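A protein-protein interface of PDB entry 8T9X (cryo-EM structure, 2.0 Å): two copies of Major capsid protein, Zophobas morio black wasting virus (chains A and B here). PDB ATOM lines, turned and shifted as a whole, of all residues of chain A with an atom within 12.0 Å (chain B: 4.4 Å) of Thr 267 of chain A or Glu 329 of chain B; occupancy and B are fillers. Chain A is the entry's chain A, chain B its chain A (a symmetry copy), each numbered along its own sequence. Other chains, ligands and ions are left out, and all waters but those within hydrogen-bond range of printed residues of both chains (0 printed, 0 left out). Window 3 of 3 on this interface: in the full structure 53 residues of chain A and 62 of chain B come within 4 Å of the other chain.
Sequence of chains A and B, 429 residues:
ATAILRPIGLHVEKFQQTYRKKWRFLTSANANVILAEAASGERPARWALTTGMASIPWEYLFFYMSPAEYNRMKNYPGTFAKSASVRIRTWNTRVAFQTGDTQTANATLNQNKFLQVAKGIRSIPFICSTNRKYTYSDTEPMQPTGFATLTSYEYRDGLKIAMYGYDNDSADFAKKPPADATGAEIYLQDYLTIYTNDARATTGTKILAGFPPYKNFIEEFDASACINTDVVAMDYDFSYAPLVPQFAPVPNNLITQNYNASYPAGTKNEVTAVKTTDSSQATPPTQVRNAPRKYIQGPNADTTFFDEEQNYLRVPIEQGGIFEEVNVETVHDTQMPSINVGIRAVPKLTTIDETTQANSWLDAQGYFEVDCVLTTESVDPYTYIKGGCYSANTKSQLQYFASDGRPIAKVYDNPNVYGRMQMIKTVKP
Of the 15 printed residues of chain A, 3 touch a printed residue of chain B. Printed residues of chain A that touch a printed residue of chain B: Gly 266, Thr 267 and Asn 269. Among the printed residues, no Asp or Glu carboxylate lies within 4 Å of a Lys or Arg side-chain nitrogen of the other chain.
Asn 269 of chain B touches its own counterpart, Asn 269 of chain A. Positions printed for both chains: 268, 269, 270, 272, 328, 329 and 330. Of the 8 pairs that touch across the chains among the printed residues, 1 has its exchanged pair printed and touching as well.
OD1 of Asn 269 of chain A sits at hydrogen-bond distance from ND2 of Asn 269 of chain B, 3.1 Å away. ND2 of Asn 269 of chain B sits at hydrogen-bond distance from O of Thr 267 of chain A (3.0 Å). N of Thr 267 of chain A is in hydrogen-bond range of O of Val 331 of chain B, 2.9 Å away.
N of Glu 325 of chain B sits at hydrogen-bond distance from OE1 of Glu 329 of chain B (2.8 Å). The backbone carbonyl oxygen (O) of Glu 329 of chain B sits at hydrogen-bond distance from the side-chain amino group (NZ) of Lys 268 of chain B, at 2.8 Å. The backbone NH (N) of Thr 272 of chain B sits at hydrogen-bond distance from the side-chain carboxylate (OE2) of Glu 324 of chain B (2.8 Å). NH2 of Arg 289 of chain A sits close to OD1 of Asn 269 of chain A, 3.4 Å away.
CA of Thr 272 of chain B touches O of Gly 266 of chain A (3.2 Å). Gly 266 of chain A touches Val 331 of chain B. Thr 267 of chain A touches Lys 268 of chain B. CG2 of Thr 267 of chain A touches O of Glu 329 of chain B, at 3.6 Å. CA of Thr 330 of chain B touches OG1 of Thr 267 of chain A, at 3.5 Å.
Thr 267 of chain A touches just these residues of chain B: Lys 268, Asn 269, Glu 329, Thr 330 and Val 331. Of chain A, only Thr 267 (3.6 Å) comes within 4 Å of Glu 329 of chain B. Asn 269 of chain B touches just these residues of chain A: Thr 267 and Asn 269. No residue of chain A comes within 4 Å of Glu 270 of chain B. No residue of chain A comes within 4 Å of Glu 324 of chain B. No residue of chain A comes within 4 Å of Val 328 of chain B. Of the printed residues of chain B, Asn 269 of chain A touches Asn 269. Printed residues of chain A within 4 Å of Lys 268 of chain B: Thr 267. Printed residues of chain B within 4 Å of Gly 266 of chain A: Thr 272 and Val 331. The nearest residue of chain A that does not touch Glu 329 of chain B is Gly 266 of chain A (7.1 Å).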
ATOM      1  N   TYR A 263      13.821  -3.070 -17.176  1.00  0.00           N
ATOM      2  CA  TYR A 263      13.145  -2.303 -18.209  1.00  0.00           C
ATOM      3  C   TYR A 263      11.658  -2.599 -18.126  1.00  0.00           C
ATOM      4  O   TYR A 263      11.257  -3.618 -17.555  1.00  0.00           O
ATOM      5  CB  TYR A 263      13.690  -2.637 -19.605  1.00  0.00           C
ATOM      6  CG  TYR A 263      14.026  -4.089 -19.810  1.00  0.00           C
ATOM      7  CD1 TYR A 263      13.081  -4.969 -20.309  1.00  0.00           C
ATOM      8  CD2 TYR A 263      15.292  -4.579 -19.521  1.00  0.00           C
ATOM      9  CE1 TYR A 263      13.379  -6.297 -20.500  1.00  0.00           C
ATOM     10  CE2 TYR A 263      15.600  -5.905 -19.712  1.00  0.00           C
ATOM     11  CZ  TYR A 263      14.637  -6.760 -20.202  1.00  0.00           C
ATOM     12  OH  TYR A 263      14.929  -8.082 -20.400  1.00  0.00           O
ATOM     13  N   PRO A 264      10.815  -1.726 -18.675  1.00  0.00           N
ATOM     14  CA  PRO A 264       9.367  -1.949 -18.588  1.00  0.00           C
ATOM     15  C   PRO A 264       8.932  -3.213 -19.315  1.00  0.00           C
ATOM     16  O   PRO A 264       9.465  -3.561 -20.369  1.00  0.00           O
ATOM     17  CB  PRO A 264       8.780  -0.697 -19.251  1.00  0.00           C
ATOM     18  CG  PRO A 264       9.857   0.315 -19.180  1.00  0.00           C
ATOM     19  CD  PRO A 264      11.123  -0.450 -19.340  1.00  0.00           C
ATOM     20  N   ALA A 265       7.951  -3.898 -18.738  1.00  0.00           N
ATOM     21  CA  ALA A 265       7.202  -4.920 -19.453  1.00  0.00           C
ATOM     22  C   ALA A 265       5.815  -4.446 -19.858  1.00  0.00           C
ATOM     23  O   ALA A 265       5.117  -5.164 -20.580  1.00  0.00           O
ATOM     24  CB  ALA A 265       7.077  -6.189 -18.605  1.00  0.00           C
ATOM     25  N   GLY A 266       5.409  -3.257 -19.423  1.00  0.00           N
ATOM     26  CA  GLY A 266       4.067  -2.788 -19.706  1.00  0.00           C
ATOM     27  C   GLY A 266       3.030  -3.685 -19.065  1.00  0.00           C
ATOM     28  O   GLY A 266       3.201  -4.174 -17.946  1.00  0.00           O
ATOM     29  N   THR A 267       1.938  -3.908 -19.785  1.00  0.00           N
ATOM     30  CA  THR A 267       0.878  -4.799 -19.335  1.00  0.00           C
ATOM     31  C   THR A 267       1.022  -6.209 -19.889  1.00  0.00           C
ATOM     32  O   THR A 267       0.149  -7.046 -19.653  1.00  0.00           O
ATOM     33  CB  THR A 267      -0.492  -4.222 -19.715  1.00  0.00           C
ATOM     34  OG1 THR A 267      -0.515  -3.916 -21.114  1.00  0.00           O
ATOM     35  CG2 THR A 267      -0.771  -2.960 -18.922  1.00  0.00           C
ATOM     36  N   LYS A 268       2.097  -6.486 -20.617  1.00  0.00           N
ATOM     37  CA  LYS A 268       2.335  -7.821 -21.147  1.00  0.00           C
ATOM     38  C   LYS A 268       2.956  -8.717 -20.082  1.00  0.00           C
ATOM     39  O   LYS A 268       3.770  -8.273 -19.271  1.00  0.00           O
ATOM     40  CB  LYS A 268       3.251  -7.736 -22.369  1.00  0.00           C
ATOM     41  CG  LYS A 268       3.684  -9.069 -22.960  1.00  0.00           C
ATOM     42  CD  LYS A 268       2.511  -9.854 -23.517  1.00  0.00           C
ATOM     43  CE  LYS A 268       2.984 -11.061 -24.321  1.00  0.00           C
ATOM     44  NZ  LYS A 268       3.075 -12.295 -23.495  1.00  0.00           N
ATOM     45  N   ASN A 269       2.562  -9.986 -20.082  1.00  0.00           N
ATOM     46  CA  ASN A 269       3.242 -10.993 -19.277  1.00  0.00           C
ATOM     47  C   ASN A 269       4.406 -11.546 -20.089  1.00  0.00           C
ATOM     48  O   ASN A 269       4.203 -12.158 -21.141  1.00  0.00           O
ATOM     49  CB  ASN A 269       2.282 -12.106 -18.865  1.00  0.00           C
ATOM     50  CG  ASN A 269       1.330 -11.684 -17.767  1.00  0.00           C
ATOM     51  OD1 ASN A 269       1.679 -10.891 -16.899  1.00  0.00           O
ATOM     52  ND2 ASN A 269       0.120 -12.224 -17.796  1.00  0.00           N
ATOM     53  N   GLU A 270       5.628 -11.313 -19.616  1.00  0.00           N
ATOM     54  CA  GLU A 270       6.813 -11.849 -20.272  1.00  0.00           C
ATOM     55  C   GLU A 270       7.449 -12.992 -19.499  1.00  0.00           C
ATOM     56  O   GLU A 270       8.283 -13.710 -20.060  1.00  0.00           O
ATOM     57  CB  GLU A 270       7.852 -10.744 -20.490  1.00  0.00           C
ATOM     58  CG  GLU A 270       7.599  -9.910 -21.729  1.00  0.00           C
ATOM     59  CD  GLU A 270       8.378  -8.612 -21.735  1.00  0.00           C
ATOM     60  OE1 GLU A 270       9.592  -8.642 -21.448  1.00  0.00           O
ATOM     61  OE2 GLU A 270       7.775  -7.559 -22.032  1.00  0.00           O
ATOM     62  N   VAL A 271       7.080 -13.168 -18.236  1.00  0.00           N
ATOM     63  CA  VAL A 271       7.502 -14.297 -17.421  1.00  0.00           C
ATOM     64  C   VAL A 271       6.284 -15.178 -17.185  1.00  0.00           C
ATOM     65  O   VAL A 271       5.208 -14.681 -16.839  1.00  0.00           O
ATOM     66  CB  VAL A 271       8.123 -13.832 -16.090  1.00  0.00           C
ATOM     67  CG1 VAL A 271       8.507 -15.022 -15.228  1.00  0.00           C
ATOM     68  CG2 VAL A 271       9.329 -12.938 -16.344  1.00  0.00           C
ATOM     69  N   THR A 272       6.449 -16.481 -17.387  1.00  0.00           N
ATOM     70  CA  THR A 272       5.328 -17.402 -17.293  1.00  0.00           C
ATOM     71  C   THR A 272       4.923 -17.620 -15.837  1.00  0.00           C
ATOM     72  O   THR A 272       5.626 -17.243 -14.899  1.00  0.00           O
ATOM     73  CB  THR A 272       5.665 -18.741 -17.947  1.00  0.00           C
ATOM     74  OG1 THR A 272       6.687 -19.401 -17.193  1.00  0.00           O
ATOM     75  CG2 THR A 272       6.134 -18.537 -19.374  1.00  0.00           C
ATOM     76  N   GLN A 287      -2.414 -18.690  -9.126  1.00  0.00           N
ATOM     77  CA  GLN A 287      -1.479 -18.473 -10.223  1.00  0.00           C
ATOM     78  C   GLN A 287      -0.263 -17.734  -9.687  1.00  0.00           C
ATOM     79  O   GLN A 287      -0.399 -16.644  -9.121  1.00  0.00           O
ATOM     80  CB  GLN A 287      -2.146 -17.691 -11.352  1.00  0.00           C
ATOM     81  CG  GLN A 287      -1.252 -17.385 -12.522  1.00  0.00           C
ATOM     82  CD  GLN A 287      -1.949 -16.546 -13.565  1.00  0.00           C
ATOM     83  OE1 GLN A 287      -3.045 -16.880 -14.006  1.00  0.00           O
ATOM     84  NE2 GLN A 287      -1.323 -15.445 -13.958  1.00  0.00           N
ATOM     85  N   ARG A 289       3.585 -16.281 -10.573  1.00  0.00           N
ATOM     86  CA  ARG A 289       4.606 -15.917 -11.542  1.00  0.00           C
ATOM     87  C   ARG A 289       5.996 -16.071 -10.922  1.00  0.00           C
ATOM     88  O   ARG A 289       6.150 -16.179  -9.704  1.00  0.00           O
ATOM     89  CB  ARG A 289       4.389 -14.482 -12.033  1.00  0.00           C
ATOM     90  CG  ARG A 289       5.071 -14.143 -13.354  1.00  0.00           C
ATOM     91  CD  ARG A 289       4.521 -12.869 -13.989  1.00  0.00           C
ATOM     92  NE  ARG A 289       3.070 -12.759 -13.914  1.00  0.00           N
ATOM     93  CZ  ARG A 289       2.224 -13.408 -14.703  1.00  0.00           C
ATOM     94  NH1 ARG A 289       2.651 -14.207 -15.666  1.00  0.00           N
ATOM     95  NH2 ARG A 289       0.919 -13.243 -14.527  1.00  0.00           N
ATOM     96  N   VAL A 328      10.399 -11.223 -25.379  1.00  0.00           N
ATOM     97  CA  VAL A 328       8.973 -10.980 -25.183  1.00  0.00           C
ATOM     98  C   VAL A 328       8.215 -12.170 -25.755  1.00  0.00           C
ATOM     99  O   VAL A 328       7.959 -12.239 -26.961  1.00  0.00           O
ATOM    100  CB  VAL A 328       8.521  -9.663 -25.845  1.00  0.00           C
ATOM    101  CG1 VAL A 328       7.052  -9.399 -25.557  1.00  0.00           C
ATOM    102  CG2 VAL A 328       9.375  -8.498 -25.376  1.00  0.00           C
ATOM    103  N   GLU A 329       7.847 -13.108 -24.893  1.00  0.00           N
ATOM    104  CA  GLU A 329       7.338 -14.401 -25.319  1.00  0.00           C
ATOM    105  C   GLU A 329       5.842 -14.520 -25.059  1.00  0.00           C
ATOM    106  O   GLU A 329       5.283 -13.837 -24.200  1.00  0.00           O
ATOM    107  CB  GLU A 329       8.073 -15.522 -24.583  1.00  0.00           C
ATOM    108  CG  GLU A 329       7.972 -15.405 -23.067  1.00  0.00           C
ATOM    109  CD  GLU A 329       8.756 -16.472 -22.334  1.00  0.00           C
ATOM    110  OE1 GLU A 329       9.290 -17.383 -22.997  1.00  0.00           O
ATOM    111  OE2 GLU A 329       8.834 -16.402 -21.092  1.00  0.00           O
ATOM    112  N   THR A 330       5.200 -15.405 -25.814  1.00  0.00           N
ATOM    113  CA  THR A 330       3.818 -15.796 -25.577  1.00  0.00           C
ATOM    114  C   THR A 330       3.772 -17.309 -25.431  1.00  0.00           C
ATOM    115  O   THR A 330       4.144 -18.035 -26.358  1.00  0.00           O
ATOM    116  CB  THR A 330       2.901 -15.339 -26.715  1.00  0.00           C
ATOM    117  OG1 THR A 330       2.825 -13.909 -26.724  1.00  0.00           O
ATOM    118  CG2 THR A 330       1.505 -15.908 -26.530  1.00  0.00           C
ATOM    119  N   LYS B 268      -7.328  -9.171 -17.259  1.00  0.00           N
ATOM    120  CA  LYS B 268      -6.533  -8.131 -17.894  1.00  0.00           C
ATOM    121  C   LYS B 268      -5.506  -7.571 -16.918  1.00  0.00           C
ATOM    122  O   LYS B 268      -5.769  -7.434 -15.722  1.00  0.00           O
ATOM    123  CB  LYS B 268      -7.449  -7.014 -18.397  1.00  0.00           C
ATOM    124  CG  LYS B 268      -6.746  -5.798 -18.981  1.00  0.00           C
ATOM    125  CD  LYS B 268      -5.967  -6.139 -20.238  1.00  0.00           C
ATOM    126  CE  LYS B 268      -5.477  -4.879 -20.945  1.00  0.00           C
ATOM    127  NZ  LYS B 268      -4.106  -4.485 -20.521  1.00  0.00           N
ATOM    128  N   ASN B 269      -4.322  -7.251 -17.432  1.00  0.00           N
ATOM    129  CA  ASN B 269      -3.339  -6.497 -16.664  1.00  0.00           C
ATOM    130  C   ASN B 269      -3.619  -5.013 -16.858  1.00  0.00           C
ATOM    131  O   ASN B 269      -3.519  -4.496 -17.974  1.00  0.00           O
ATOM    132  CB  ASN B 269      -1.918  -6.849 -17.097  1.00  0.00           C
ATOM    133  CG  ASN B 269      -1.468  -8.201 -16.590  1.00  0.00           C
ATOM    134  OD1 ASN B 269      -1.848  -8.628 -15.505  1.00  0.00           O
ATOM    135  ND2 ASN B 269      -0.643  -8.880 -17.375  1.00  0.00           N
ATOM    136  N   GLU B 270      -3.991  -4.328 -15.779  1.00  0.00           N
ATOM    137  CA  GLU B 270      -4.222  -2.891 -15.831  1.00  0.00           C
ATOM    138  C   GLU B 270      -3.126  -2.093 -15.146  1.00  0.00           C
ATOM    139  O   GLU B 270      -3.049  -0.876 -15.346  1.00  0.00           O
ATOM    140  CB  GLU B 270      -5.574  -2.542 -15.199  1.00  0.00           C
ATOM    141  CG  GLU B 270      -6.746  -2.717 -16.143  1.00  0.00           C
ATOM    142  CD  GLU B 270      -8.081  -2.745 -15.426  1.00  0.00           C
ATOM    143  OE1 GLU B 270      -8.316  -1.870 -14.567  1.00  0.00           O
ATOM    144  OE2 GLU B 270      -8.897  -3.640 -15.727  1.00  0.00           O
ATOM    145  N   THR B 272       1.054  -1.897 -14.786  1.00  0.00           N
ATOM    146  CA  THR B 272       2.223  -2.360 -15.517  1.00  0.00           C
ATOM    147  C   THR B 272       3.191  -3.088 -14.589  1.00  0.00           C
ATOM    148  O   THR B 272       3.076  -3.052 -13.363  1.00  0.00           O
ATOM    149  CB  THR B 272       2.933  -1.195 -16.203  1.00  0.00           C
ATOM    150  OG1 THR B 272       3.496  -0.324 -15.215  1.00  0.00           O
ATOM    151  CG2 THR B 272       1.969  -0.419 -17.078  1.00  0.00           C
ATOM    152  N   GLU B 324       2.040   5.435 -16.417  1.00  0.00           N
ATOM    153  CA  GLU B 324       0.774   4.725 -16.346  1.00  0.00           C
ATOM    154  C   GLU B 324      -0.377   5.720 -16.329  1.00  0.00           C
ATOM    155  O   GLU B 324      -0.234   6.854 -15.867  1.00  0.00           O
ATOM    156  CB  GLU B 324       0.674   3.841 -15.097  1.00  0.00           C
ATOM    157  CG  GLU B 324       1.681   2.714 -14.998  1.00  0.00           C
ATOM    158  CD  GLU B 324       1.353   1.760 -13.858  1.00  0.00           C
ATOM    159  OE1 GLU B 324       0.589   2.154 -12.956  1.00  0.00           O
ATOM    160  OE2 GLU B 324       1.868   0.626 -13.849  1.00  0.00           O
ATOM    161  N   GLU B 325      -1.519   5.281 -16.839  1.00  0.00           N
ATOM    162  CA  GLU B 325      -2.778   5.987 -16.687  1.00  0.00           C
ATOM    163  C   GLU B 325      -3.747   5.079 -15.942  1.00  0.00           C
ATOM    164  O   GLU B 325      -3.702   3.856 -16.082  1.00  0.00           O
ATOM    165  CB  GLU B 325      -3.354   6.406 -18.042  1.00  0.00           C
ATOM    166  CG  GLU B 325      -2.482   7.391 -18.795  1.00  0.00           C
ATOM    167  CD  GLU B 325      -3.107   7.865 -20.092  1.00  0.00           C
ATOM    168  OE1 GLU B 325      -4.122   7.279 -20.519  1.00  0.00           O
ATOM    169  OE2 GLU B 325      -2.577   8.825 -20.687  1.00  0.00           O
ATOM    170  N   ASN B 327      -6.754   4.303 -16.210  1.00  0.00           N
ATOM    171  CA  ASN B 327      -7.799   3.587 -16.927  1.00  0.00           C
ATOM    172  C   ASN B 327      -7.370   2.147 -17.223  1.00  0.00           C
ATOM    173  O   ASN B 327      -6.326   1.668 -16.775  1.00  0.00           O
ATOM    174  CB  ASN B 327      -8.137   4.317 -18.221  1.00  0.00           C
ATOM    175  CG  ASN B 327      -6.903   4.728 -18.993  1.00  0.00           C
ATOM    176  OD1 ASN B 327      -6.200   3.889 -19.550  1.00  0.00           O
ATOM    177  ND2 ASN B 327      -6.642   6.025 -19.043  1.00  0.00           N
ATOM    178  N   VAL B 328      -8.201   1.446 -17.995  1.00  0.00           N
ATOM    179  CA  VAL B 328      -7.857   0.127 -18.516  1.00  0.00           C
ATOM    180  C   VAL B 328      -6.881   0.322 -19.669  1.00  0.00           C
ATOM    181  O   VAL B 328      -7.286   0.582 -20.807  1.00  0.00           O
ATOM    182  CB  VAL B 328      -9.107  -0.652 -18.974  1.00  0.00           C
ATOM    183  CG1 VAL B 328      -8.725  -2.047 -19.436  1.00  0.00           C
ATOM    184  CG2 VAL B 328     -10.139  -0.721 -17.861  1.00  0.00           C
ATOM    185  N   GLU B 329      -5.593   0.192 -19.384  1.00  0.00           N
ATOM    186  CA  GLU B 329      -4.545   0.584 -20.311  1.00  0.00           C
ATOM    187  C   GLU B 329      -3.849  -0.633 -20.906  1.00  0.00           C
ATOM    188  O   GLU B 329      -3.849  -1.720 -20.327  1.00  0.00           O
ATOM    189  CB  GLU B 329      -3.516   1.462 -19.600  1.00  0.00           C
ATOM    190  CG  GLU B 329      -2.896   0.786 -18.382  1.00  0.00           C
ATOM    191  CD  GLU B 329      -1.928   1.679 -17.635  1.00  0.00           C
ATOM    192  OE1 GLU B 329      -1.641   2.789 -18.123  1.00  0.00           O
ATOM    193  OE2 GLU B 329      -1.451   1.265 -16.560  1.00  0.00           O
ATOM    194  N   THR B 330      -3.247  -0.433 -22.073  1.00  0.00           N
ATOM    195  CA  THR B 330      -2.371  -1.417 -22.693  1.00  0.00           C
ATOM    196  C   THR B 330      -1.030  -0.752 -22.966  1.00  0.00           C
ATOM    197  O   THR B 330      -0.964   0.233 -23.708  1.00  0.00           O
ATOM    198  CB  THR B 330      -2.970  -1.966 -23.991  1.00  0.00           C
ATOM    199  OG1 THR B 330      -4.141  -2.736 -23.689  1.00  0.00           O
ATOM    200  CG2 THR B 330      -1.965  -2.854 -24.702  1.00  0.00           C
ATOM    201  N   VAL B 331       0.030  -1.286 -22.367  1.00  0.00           N
ATOM    202  CA  VAL B 331       1.347  -0.663 -22.389  1.00  0.00           C
ATOM    203  C   VAL B 331       2.376  -1.686 -22.846  1.00  0.00           C
ATOM    204  O   VAL B 331       2.342  -2.847 -22.425  1.00  0.00           O
ATOM    205  CB  VAL B 331       1.732  -0.095 -21.005  1.00  0.00           C
ATOM    206  CG1 VAL B 331       3.067   0.622 -21.074  1.00  0.00           C
ATOM    207  CG2 VAL B 331       0.649   0.833 -20.479  1.00  0.00           C
